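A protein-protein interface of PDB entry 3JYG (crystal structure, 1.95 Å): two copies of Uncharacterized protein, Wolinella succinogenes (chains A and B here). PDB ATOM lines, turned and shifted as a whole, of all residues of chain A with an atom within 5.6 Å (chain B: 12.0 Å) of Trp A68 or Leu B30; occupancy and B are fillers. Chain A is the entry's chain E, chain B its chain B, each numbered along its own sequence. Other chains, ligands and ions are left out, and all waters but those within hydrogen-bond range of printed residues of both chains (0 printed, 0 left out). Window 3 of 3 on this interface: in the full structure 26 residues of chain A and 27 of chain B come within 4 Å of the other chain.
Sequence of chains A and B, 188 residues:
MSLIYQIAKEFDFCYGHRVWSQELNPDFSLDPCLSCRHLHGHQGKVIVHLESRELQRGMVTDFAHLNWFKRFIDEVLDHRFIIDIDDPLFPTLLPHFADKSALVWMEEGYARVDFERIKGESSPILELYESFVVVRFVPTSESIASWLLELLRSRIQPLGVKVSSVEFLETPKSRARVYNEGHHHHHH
NE2 of His A65 sits at hydrogen-bond distance from N of Asn B25, 2.9 Å away. The backbone NH (N) of Trp A68 lies within hydrogen-bond range of the backbone carbonyl oxygen (O) of Phe B28, 3.2 Å away. O of Ser B29 is in hydrogen-bond range of ND2 of Asn A67, 2.9 Å away. The backbone carbonyl oxygen (O) of Ala A64 sits close to the backbone carbonyl oxygen (O) of Phe B28, at 3.4 Å.
OD1 of Asn B25 sits at hydrogen-bond distance from N of Asp B27, 3.1 Å away. OG of Ser B29 lies within hydrogen-bond range of O of Asp B31 (2.8 Å). O of Ala A64 sits close to ND2 of Asn A67 (3.4 Å). The indole nitrogen of Trp A68 sits at hydrogen-bond distance from the backbone carbonyl oxygen of His A65 (2.9 Å).
Ala A64 touches Ser B29 (O to CA, 3.1 Å). Leu B24 touches His A65 (CA to NE2, 3.7 Å). His A65 touches Phe B28. N of Asn A67 touches O of Phe B28, 3.6 Å away. Asn A67 touches Leu B30. Trp A68 touches Leu B30 (CB to CD1, 3.7 Å). NE of Arg A71 touches CD2 of Leu B30, at 3.4 Å. Arg A155 touches Phe B28 (O to CE2, 3.3 Å).
Of chain B, only Phe B28 (3.2 Å) and Leu B30 (3.7 Å) come within 4 Å of Trp A68. No residue of chain B comes within 4 Å of Phe A69. Arg A71 touches just one residue of chain B: Leu B30. No residue of chain B comes within 4 Å of Leu A151. Leu A152 touches none of the printed residues of chain B. Of the printed residues of chain B, Arg A155 touches Phe B28 (3.3 Å). No residue of chain B comes within 4 Å of Ile A156. Of the printed residues of chain A, Leu B24 touches His A65 (3.7 Å). Of the printed residues of chain A, Phe B28 touches Ala A64 (3.4 Å), His A65 (3.5 Å), Asn A67 (3.6 Å), Trp A68 (3.2 Å) and Arg A155 (3.3 Å). Printed residues of chain A within 4 Å of Ser B29: Ala A64 (3.1 Å) and Asn A67 (2.9 Å). Leu B30 touches just these residues of chain A: Asn A67 (3.7 Å), Trp A68 (3.7 Å) and Arg A71 (3.4 Å). The nearest residue of chain B that does not touch Trp A68 is Asp B27 (4.5 Å). The nearest residue of chain A that does not touch Leu B30 is Ala A64 (5.3 Å). The nearest printed residue of chain A that does not touch Leu B24 is Ala A64 (4.1 Å).
Of the 14 printed residues of chain A, 6 touch a printed residue of chain B. Printed residues of chain A that touch a printed residue of chain B: Ala A64, His A65, Asn A67, Trp A68, Arg A71 and Arg A155. Hydrophobic or aromatic side chains of chain A that line the printed part of chain B: Ala A64, His A65 and Trp A68. Hydrophobic or aromatic side chains of chain B that line the printed part of chain A: Leu B24, Phe B28 and Leu B30. Among the printed residues, 12 pairs touch across the chains. Among the printed residues, no Asp or Glu carboxylate lies within 4 Å of a Lys or Arg side-chain nitrogen of the other chain.
No position is printed for both chains. Of the 12 pairs that touch across the chains among the printed residues, none has its exchanged pair printed and touching as well.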
ATOM      1  N   ALA A  64      -0.693 -11.961  25.918  1.00  0.00           N
ATOM      2  CA  ALA A  64      -1.324 -10.911  25.069  1.00  0.00           C
ATOM      3  C   ALA A  64      -0.363 -10.220  24.138  1.00  0.00           C
ATOM      4  O   ALA A  64      -0.782  -9.580  23.180  1.00  0.00           O
ATOM      5  CB  ALA A  64      -2.089  -9.848  25.915  1.00  0.00           C
ATOM      6  N   HIS A  65       0.941 -10.377  24.387  1.00  0.00           N
ATOM      7  CA  HIS A  65       1.965  -9.804  23.498  1.00  0.00           C
ATOM      8  C   HIS A  65       2.112 -10.500  22.123  1.00  0.00           C
ATOM      9  O   HIS A  65       2.904 -10.070  21.279  1.00  0.00           O
ATOM     10  CB  HIS A  65       3.315  -9.719  24.216  1.00  0.00           C
ATOM     11  CG  HIS A  65       3.366  -8.659  25.282  1.00  0.00           C
ATOM     12  ND1 HIS A  65       4.171  -8.764  26.400  1.00  0.00           N
ATOM     13  CD2 HIS A  65       2.692  -7.489  25.413  1.00  0.00           C
ATOM     14  CE1 HIS A  65       4.039  -7.671  27.141  1.00  0.00           C
ATOM     15  NE2 HIS A  65       3.145  -6.879  26.568  1.00  0.00           N
ATOM     16  N   LEU A  66       1.314 -11.548  21.910  1.00  0.00           N
ATOM     17  CA  LEU A  66       1.162 -12.163  20.587  1.00  0.00           C
ATOM     18  C   LEU A  66      -0.138 -11.760  19.899  1.00  0.00           C
ATOM     19  O   LEU A  66      -0.458 -12.303  18.822  1.00  0.00           O
ATOM     20  CB  LEU A  66       1.222 -13.684  20.685  1.00  0.00           C
ATOM     21  CG  LEU A  66       2.649 -14.215  20.925  1.00  0.00           C
ATOM     22  CD1 LEU A  66       2.695 -15.668  21.480  1.00  0.00           C
ATOM     23  CD2 LEU A  66       3.532 -14.046  19.652  1.00  0.00           C
ATOM     24  N   ASN A  67      -0.880 -10.817  20.494  1.00  0.00           N
ATOM     25  CA  ASN A  67      -2.170 -10.396  19.897  1.00  0.00           C
ATOM     26  C   ASN A  67      -1.970  -9.870  18.485  1.00  0.00           C
ATOM     27  O   ASN A  67      -2.846 -10.053  17.647  1.00  0.00           O
ATOM     28  CB  ASN A  67      -2.896  -9.350  20.761  1.00  0.00           C
ATOM     29  CG  ASN A  67      -3.622  -9.975  21.957  1.00  0.00           C
ATOM     30  OD1 ASN A  67      -3.681 -11.183  22.094  1.00  0.00           O
ATOM     31  ND2 ASN A  67      -4.166  -9.137  22.826  1.00  0.00           N
ATOM     32  N   TRP A  68      -0.807  -9.250  18.221  1.00  0.00           N
ATOM     33  CA  TRP A  68      -0.468  -8.746  16.840  1.00  0.00           C
ATOM     34  C   TRP A  68      -0.306  -9.911  15.858  1.00  0.00           C
ATOM     35  O   TRP A  68      -0.685  -9.828  14.683  1.00  0.00           O
ATOM     36  CB  TRP A  68       0.809  -7.889  16.838  1.00  0.00           C
ATOM     37  CG  TRP A  68       1.977  -8.720  17.205  1.00  0.00           C
ATOM     38  CD1 TRP A  68       2.383  -9.047  18.466  1.00  0.00           C
ATOM     39  CD2 TRP A  68       2.853  -9.417  16.305  1.00  0.00           C
ATOM     40  NE1 TRP A  68       3.462  -9.889  18.409  1.00  0.00           N
ATOM     41  CE2 TRP A  68       3.770 -10.142  17.100  1.00  0.00           C
ATOM     42  CE3 TRP A  68       2.929  -9.521  14.910  1.00  0.00           C
ATOM     43  CZ2 TRP A  68       4.766 -10.953  16.552  1.00  0.00           C
ATOM     44  CZ3 TRP A  68       3.918 -10.329  14.357  1.00  0.00           C
ATOM     45  CH2 TRP A  68       4.814 -11.048  15.182  1.00  0.00           C
ATOM     46  N   PHE A  69       0.246 -11.008  16.367  1.00  0.00           N
ATOM     47  CA  PHE A  69       0.409 -12.232  15.592  1.00  0.00           C
ATOM     48  C   PHE A  69      -0.941 -12.893  15.355  1.00  0.00           C
ATOM     49  O   PHE A  69      -1.216 -13.332  14.226  1.00  0.00           O
ATOM     50  CB  PHE A  69       1.403 -13.187  16.286  1.00  0.00           C
ATOM     51  CG  PHE A  69       1.709 -14.424  15.491  1.00  0.00           C
ATOM     52  CD1 PHE A  69       2.573 -14.367  14.398  1.00  0.00           C
ATOM     53  CD2 PHE A  69       1.118 -15.651  15.833  1.00  0.00           C
ATOM     54  CE1 PHE A  69       2.837 -15.522  13.618  1.00  0.00           C
ATOM     55  CE2 PHE A  69       1.361 -16.814  15.073  1.00  0.00           C
ATOM     56  CZ  PHE A  69       2.245 -16.759  13.970  1.00  0.00           C
ATOM     57  N   LYS A  70      -1.802 -12.950  16.381  1.00  0.00           N
ATOM     58  CA  LYS A  70      -3.172 -13.467  16.162  1.00  0.00           C
ATOM     59  C   LYS A  70      -3.914 -12.671  15.051  1.00  0.00           C
ATOM     60  O   LYS A  70      -4.582 -13.261  14.176  1.00  0.00           O
ATOM     61  CB  LYS A  70      -4.009 -13.424  17.433  1.00  0.00           C
ATOM     62  CG  LYS A  70      -5.415 -14.040  17.244  1.00  0.00           C
ATOM     63  CD  LYS A  70      -6.207 -14.115  18.543  1.00  0.00           C
ATOM     64  CE  LYS A  70      -7.404 -15.053  18.356  1.00  0.00           C
ATOM     65  NZ  LYS A  70      -8.406 -14.467  17.421  1.00  0.00           N
ATOM     66  N   ARG A  71      -3.755 -11.349  15.073  1.00  0.00           N
ATOM     67  CA  ARG A  71      -4.361 -10.475  14.072  1.00  0.00           C
ATOM     68  C   ARG A  71      -3.840 -10.791  12.659  1.00  0.00           C
ATOM     69  O   ARG A  71      -4.632 -10.931  11.701  1.00  0.00           O
ATOM     70  CB  ARG A  71      -4.147  -8.998  14.436  1.00  0.00           C
ATOM     71  CG  ARG A  71      -4.828  -7.988  13.474  1.00  0.00           C
ATOM     72  CD  ARG A  71      -4.698  -6.491  13.916  1.00  0.00           C
ATOM     73  NE  ARG A  71      -3.286  -6.155  14.142  1.00  0.00           N
ATOM     74  CZ  ARG A  71      -2.760  -4.931  14.275  1.00  0.00           C
ATOM     75  NH1 ARG A  71      -3.515  -3.840  14.214  1.00  0.00           N
ATOM     76  NH2 ARG A  71      -1.451  -4.814  14.478  1.00  0.00           N
ATOM     77  N   PHE A  72      -2.513 -10.887  12.537  1.00  0.00           N
ATOM     78  CA  PHE A  72      -1.894 -11.326  11.296  1.00  0.00           C
ATOM     79  C   PHE A  72      -2.464 -12.651  10.763  1.00  0.00           C
ATOM     80  O   PHE A  72      -2.863 -12.734   9.583  1.00  0.00           O
ATOM     81  CB  PHE A  72      -0.368 -11.405  11.418  1.00  0.00           C
ATOM     82  CG  PHE A  72       0.296 -11.969  10.193  1.00  0.00           C
ATOM     83  CD1 PHE A  72       0.443 -11.184   9.036  1.00  0.00           C
ATOM     84  CD2 PHE A  72       0.785 -13.276  10.186  1.00  0.00           C
ATOM     85  CE1 PHE A  72       1.065 -11.683   7.905  1.00  0.00           C
ATOM     86  CE2 PHE A  72       1.391 -13.800   9.030  1.00  0.00           C
ATOM     87  CZ  PHE A  72       1.517 -13.001   7.896  1.00  0.00           C
ATOM     88  N   ILE A  73      -2.511 -13.681  11.607  1.00  0.00           N
ATOM     89  CA  ILE A  73      -3.179 -14.942  11.227  1.00  0.00           C
ATOM     90  C   ILE A  73      -4.648 -14.744  10.756  1.00  0.00           C
ATOM     91  O   ILE A  73      -5.084 -15.260   9.681  1.00  0.00           O
ATOM     92  CB  ILE A  73      -3.142 -16.002  12.385  1.00  0.00           C
ATOM     93  CG1 ILE A  73      -1.692 -16.401  12.795  1.00  0.00           C
ATOM     94  CG2 ILE A  73      -3.804 -17.274  11.944  1.00  0.00           C
ATOM     95  CD1 ILE A  73      -0.824 -16.659  11.636  1.00  0.00           C
ATOM     96  N   LEU A 151       9.054 -14.502  10.791  1.00  0.00           N
ATOM     97  CA  LEU A 151       8.270 -13.323  11.139  1.00  0.00           C
ATOM     98  C   LEU A 151       8.324 -13.019  12.670  1.00  0.00           C
ATOM     99  O   LEU A 151       8.500 -11.869  13.072  1.00  0.00           O
ATOM    100  CB  LEU A 151       6.804 -13.482  10.689  1.00  0.00           C
ATOM    101  CG  LEU A 151       5.835 -12.442  11.264  1.00  0.00           C
ATOM    102  CD1 LEU A 151       6.179 -11.004  10.783  1.00  0.00           C
ATOM    103  CD2 LEU A 151       4.357 -12.813  10.945  1.00  0.00           C
ATOM    104  N   LEU A 152       8.118 -14.045  13.496  1.00  0.00           N
ATOM    105  CA  LEU A 152       8.138 -13.880  14.955  1.00  0.00           C
ATOM    106  C   LEU A 152       9.500 -13.384  15.515  1.00  0.00           C
ATOM    107  O   LEU A 152       9.547 -12.420  16.333  1.00  0.00           O
ATOM    108  CB  LEU A 152       7.713 -15.206  15.611  1.00  0.00           C
ATOM    109  CG  LEU A 152       6.203 -15.461  15.483  1.00  0.00           C
ATOM    110  CD1 LEU A 152       5.882 -16.959  15.571  1.00  0.00           C
ATOM    111  CD2 LEU A 152       5.428 -14.613  16.519  1.00  0.00           C
ATOM    112  N   ARG A 155       9.979  -9.701  14.891  1.00  0.00           N
ATOM    113  CA  ARG A 155       9.095  -8.802  15.636  1.00  0.00           C
ATOM    114  C   ARG A 155       9.222  -8.815  17.164  1.00  0.00           C
ATOM    115  O   ARG A 155       8.913  -7.826  17.785  1.00  0.00           O
ATOM    116  CB  ARG A 155       7.623  -9.104  15.327  1.00  0.00           C
ATOM    117  CG  ARG A 155       7.162  -8.796  13.955  1.00  0.00           C
ATOM    118  CD  ARG A 155       7.091  -7.307  13.686  1.00  0.00           C
ATOM    119  NE  ARG A 155       6.768  -7.126  12.268  1.00  0.00           N
ATOM    120  CZ  ARG A 155       5.537  -7.149  11.747  1.00  0.00           C
ATOM    121  NH1 ARG A 155       4.451  -7.304  12.516  1.00  0.00           N
ATOM    122  NH2 ARG A 155       5.395  -6.977  10.436  1.00  0.00           N
ATOM    123  N   ILE A 156       9.601  -9.946  17.745  1.00  0.00           N
ATOM    124  CA  ILE A 156       9.523 -10.183  19.190  1.00  0.00           C
ATOM    125  C   ILE A 156      10.722  -9.591  19.972  1.00  0.00           C
ATOM    126  O   ILE A 156      10.722  -9.534  21.223  1.00  0.00           O
ATOM    127  CB  ILE A 156       9.366 -11.706  19.424  1.00  0.00           C
ATOM    128  CG1 ILE A 156       7.917 -12.164  19.121  1.00  0.00           C
ATOM    129  CG2 ILE A 156       9.919 -12.181  20.744  1.00  0.00           C
ATOM    130  CD1 ILE A 156       6.867 -11.731  20.115  1.00  0.00           C
ATOM    131  N   GLN B  22       0.052  -7.433  36.308  1.00  0.00           N
ATOM    132  CA  GLN B  22       0.116  -7.554  34.858  1.00  0.00           C
ATOM    133  C   GLN B  22       0.366  -6.160  34.250  1.00  0.00           C
ATOM    134  O   GLN B  22      -0.309  -5.195  34.623  1.00  0.00           O
ATOM    135  CB  GLN B  22      -1.199  -8.097  34.298  1.00  0.00           C
ATOM    136  CG  GLN B  22      -1.228  -8.090  32.781  1.00  0.00           C
ATOM    137  CD  GLN B  22      -2.588  -8.426  32.160  1.00  0.00           C
ATOM    138  OE1 GLN B  22      -3.643  -7.940  32.608  1.00  0.00           O
ATOM    139  NE2 GLN B  22      -2.561  -9.247  31.086  1.00  0.00           N
ATOM    140  N   GLU B  23       1.379  -6.051  33.384  1.00  0.00           N
ATOM    141  CA  GLU B  23       1.619  -4.819  32.592  1.00  0.00           C
ATOM    142  C   GLU B  23       1.698  -5.208  31.139  1.00  0.00           C
ATOM    143  O   GLU B  23       2.152  -6.304  30.819  1.00  0.00           O
ATOM    144  CB  GLU B  23       2.939  -4.144  32.988  1.00  0.00           C
ATOM    145  CG  GLU B  23       2.896  -3.494  34.357  1.00  0.00           C
ATOM    146  CD  GLU B  23       4.269  -2.944  34.824  1.00  0.00           C
ATOM    147  OE1 GLU B  23       5.211  -2.814  34.008  1.00  0.00           O
ATOM    148  OE2 GLU B  23       4.397  -2.641  36.023  1.00  0.00           O
ATOM    149  N   LEU B  24       1.231  -4.337  30.246  1.00  0.00           N
ATOM    150  CA  LEU B  24       1.262  -4.665  28.818  1.00  0.00           C
ATOM    151  C   LEU B  24       1.894  -3.592  27.973  1.00  0.00           C
ATOM    152  O   LEU B  24       1.810  -2.397  28.287  1.00  0.00           O
ATOM    153  CB  LEU B  24      -0.142  -4.962  28.260  1.00  0.00           C
ATOM    154  CG  LEU B  24      -0.956  -6.095  28.845  1.00  0.00           C
ATOM    155  CD1 LEU B  24      -2.371  -6.110  28.190  1.00  0.00           C
ATOM    156  CD2 LEU B  24      -0.179  -7.386  28.640  1.00  0.00           C
ATOM    157  N   ASN B  25       2.529  -4.040  26.889  1.00  0.00           N
ATOM    158  CA  ASN B  25       3.030  -3.150  25.854  1.00  0.00           C
ATOM    159  C   ASN B  25       1.978  -3.142  24.722  1.00  0.00           C
ATOM    160  O   ASN B  25       1.860  -4.116  24.007  1.00  0.00           O
ATOM    161  CB  ASN B  25       4.376  -3.646  25.358  1.00  0.00           C
ATOM    162  CG  ASN B  25       5.001  -2.728  24.287  1.00  0.00           C
ATOM    163  OD1 ASN B  25       4.312  -1.952  23.628  1.00  0.00           O
ATOM    164  ND2 ASN B  25       6.312  -2.845  24.112  1.00  0.00           N
ATOM    165  N   PRO B  26       1.215  -2.042  24.576  1.00  0.00           N
ATOM    166  CA  PRO B  26       0.091  -2.037  23.623  1.00  0.00           C
ATOM    167  C   PRO B  26       0.482  -2.205  22.161  1.00  0.00           C
ATOM    168  O   PRO B  26      -0.378  -2.594  21.365  1.00  0.00           O
ATOM    169  CB  PRO B  26      -0.622  -0.689  23.876  1.00  0.00           C
ATOM    170  CG  PRO B  26       0.423   0.214  24.480  1.00  0.00           C
ATOM    171  CD  PRO B  26       1.435  -0.719  25.201  1.00  0.00           C
ATOM    172  N   ASP B  27       1.750  -1.938  21.818  1.00  0.00           N
ATOM    173  CA  ASP B  27       2.287  -2.239  20.462  1.00  0.00           C
ATOM    174  C   ASP B  27       2.156  -3.727  20.127  1.00  0.00           C
ATOM    175  O   ASP B  27       2.131  -4.138  18.933  1.00  0.00           O
ATOM    176  CB  ASP B  27       3.778  -1.875  20.396  1.00  0.00           C
ATOM    177  CG  ASP B  27       4.023  -0.359  20.455  1.00  0.00           C
ATOM    178  OD1 ASP B  27       3.038   0.406  20.490  1.00  0.00           O
ATOM    179  OD2 ASP B  27       5.195   0.056  20.485  1.00  0.00           O
ATOM    180  N   PHE B  28       2.126  -4.543  21.185  1.00  0.00           N
ATOM    181  CA  PHE B  28       2.075  -5.988  21.025  1.00  0.00           C
ATOM    182  C   PHE B  28       0.710  -6.565  21.408  1.00  0.00           C
ATOM    183  O   PHE B  28       0.173  -7.412  20.683  1.00  0.00           O
ATOM    184  CB  PHE B  28       3.226  -6.636  21.805  1.00  0.00           C
ATOM    185  CG  PHE B  28       4.583  -6.334  21.228  1.00  0.00           C
ATOM    186  CD1 PHE B  28       5.305  -5.209  21.648  1.00  0.00           C
ATOM    187  CD2 PHE B  28       5.137  -7.162  20.263  1.00  0.00           C
ATOM    188  CE1 PHE B  28       6.581  -4.918  21.119  1.00  0.00           C
ATOM    189  CE2 PHE B  28       6.409  -6.885  19.717  1.00  0.00           C
ATOM    190  CZ  PHE B  28       7.128  -5.748  20.144  1.00  0.00           C
ATOM    191  N   SER B  29       0.142  -6.094  22.530  1.00  0.00           N
ATOM    192  CA  SER B  29      -1.184  -6.530  22.931  1.00  0.00           C
ATOM    193  C   SER B  29      -2.317  -5.884  22.112  1.00  0.00           C
ATOM    194  O   SER B  29      -3.421  -6.434  22.080  1.00  0.00           O
ATOM    195  CB  SER B  29      -1.410  -6.329  24.446  1.00  0.00           C
ATOM    196  OG  SER B  29      -1.542  -4.957  24.728  1.00  0.00           O
ATOM    197  N   LEU B  30      -2.063  -4.725  21.478  1.00  0.00           N
ATOM    198  CA  LEU B  30      -3.060  -4.023  20.641  1.00  0.00           C
ATOM    199  C   LEU B  30      -4.114  -3.303  21.473  1.00  0.00           C
ATOM    200  O   LEU B  30      -4.410  -2.150  21.233  1.00  0.00           O
ATOM    201  CB  LEU B  30      -3.708  -4.965  19.599  1.00  0.00           C
ATOM    202  CG  LEU B  30      -2.904  -5.281  18.312  1.00  0.00           C
ATOM    203  CD1 LEU B  30      -1.436  -5.520  18.566  1.00  0.00           C
ATOM    204  CD2 LEU B  30      -3.482  -6.452  17.557  1.00  0.00           C
ATOM    205  N   ASP B  31      -4.652  -3.998  22.462  1.00  0.00           N
ATOM    206  CA  ASP B  31      -5.583  -3.476  23.482  1.00  0.00           C
ATOM    207  C   ASP B  31      -4.767  -3.249  24.773  1.00  0.00           C
ATOM    208  O   ASP B  31      -4.155  -4.197  25.265  1.00  0.00           O
ATOM    209  CB  ASP B  31      -6.633  -4.578  23.723  1.00  0.00           C
ATOM    210  CG  ASP B  31      -7.786  -4.143  24.626  1.00  0.00           C
ATOM    211  OD1 ASP B  31      -7.600  -3.295  25.517  1.00  0.00           O
ATOM    212  OD2 ASP B  31      -8.898  -4.674  24.435  1.00  0.00           O
ATOM    213  N   PRO B  32      -4.752  -2.017  25.334  1.00  0.00           N
ATOM    214  CA  PRO B  32      -4.030  -1.850  26.623  1.00  0.00           C
ATOM    215  C   PRO B  32      -4.755  -2.375  27.907  1.00  0.00           C
ATOM    216  O   PRO B  32      -4.175  -2.346  28.991  1.00  0.00           O
ATOM    217  CB  PRO B  32      -3.819  -0.337  26.702  1.00  0.00           C
ATOM    218  CG  PRO B  32      -5.051   0.253  25.965  1.00  0.00           C
ATOM    219  CD  PRO B  32      -5.424  -0.770  24.897  1.00  0.00           C
ATOM    220  N   CYS B  33      -5.995  -2.858  27.793  1.00  0.00           N
ATOM    221  CA  CYS B  33      -6.773  -3.276  28.981  1.00  0.00           C
ATOM    222  C   CYS B  33      -6.061  -4.388  29.796  1.00  0.00           C
ATOM    223  O   CYS B  33      -5.632  -5.423  29.224  1.00  0.00           O
ATOM    224  CB  CYS B  33      -8.216  -3.665  28.607  1.00  0.00           C
ATOM    225  SG  CYS B  33      -9.282  -4.121  30.029  1.00  0.00           S
ATOM    226  N   LEU B  34      -5.897  -4.152  31.107  1.00  0.00           N
ATOM    227  CA  LEU B  34      -5.222  -5.128  31.994  1.00  0.00           C
ATOM    228  C   LEU B  34      -6.157  -6.211  32.552  1.00  0.00           C
ATOM    229  O   LEU B  34      -6.362  -6.358  33.778  1.00  0.00           O
ATOM    230  CB  LEU B  34      -4.422  -4.410  33.073  1.00  0.00           C
ATOM    231  CG  LEU B  34      -3.419  -3.372  32.517  1.00  0.00           C
ATOM    232  CD1 LEU B  34      -2.873  -2.446  33.620  1.00  0.00           C
ATOM    233  CD2 LEU B  34      -2.286  -4.017  31.693  1.00  0.00           C
ATOM    234  N   SER B  35      -6.707  -6.993  31.629  1.00  0.00           N
ATOM    235  CA  SER B  35      -7.740  -8.021  31.920  1.00  0.00           C
ATOM    236  C   SER B  35      -7.321  -9.112  32.903  1.00  0.00           C
ATOM    237  O   SER B  35      -8.180  -9.631  33.628  1.00  0.00           O
ATOM    238  CB  SER B  35      -8.330  -8.625  30.605  1.00  0.00           C
ATOM    239  OG  SER B  35      -7.472  -9.613  30.031  1.00  0.00           O
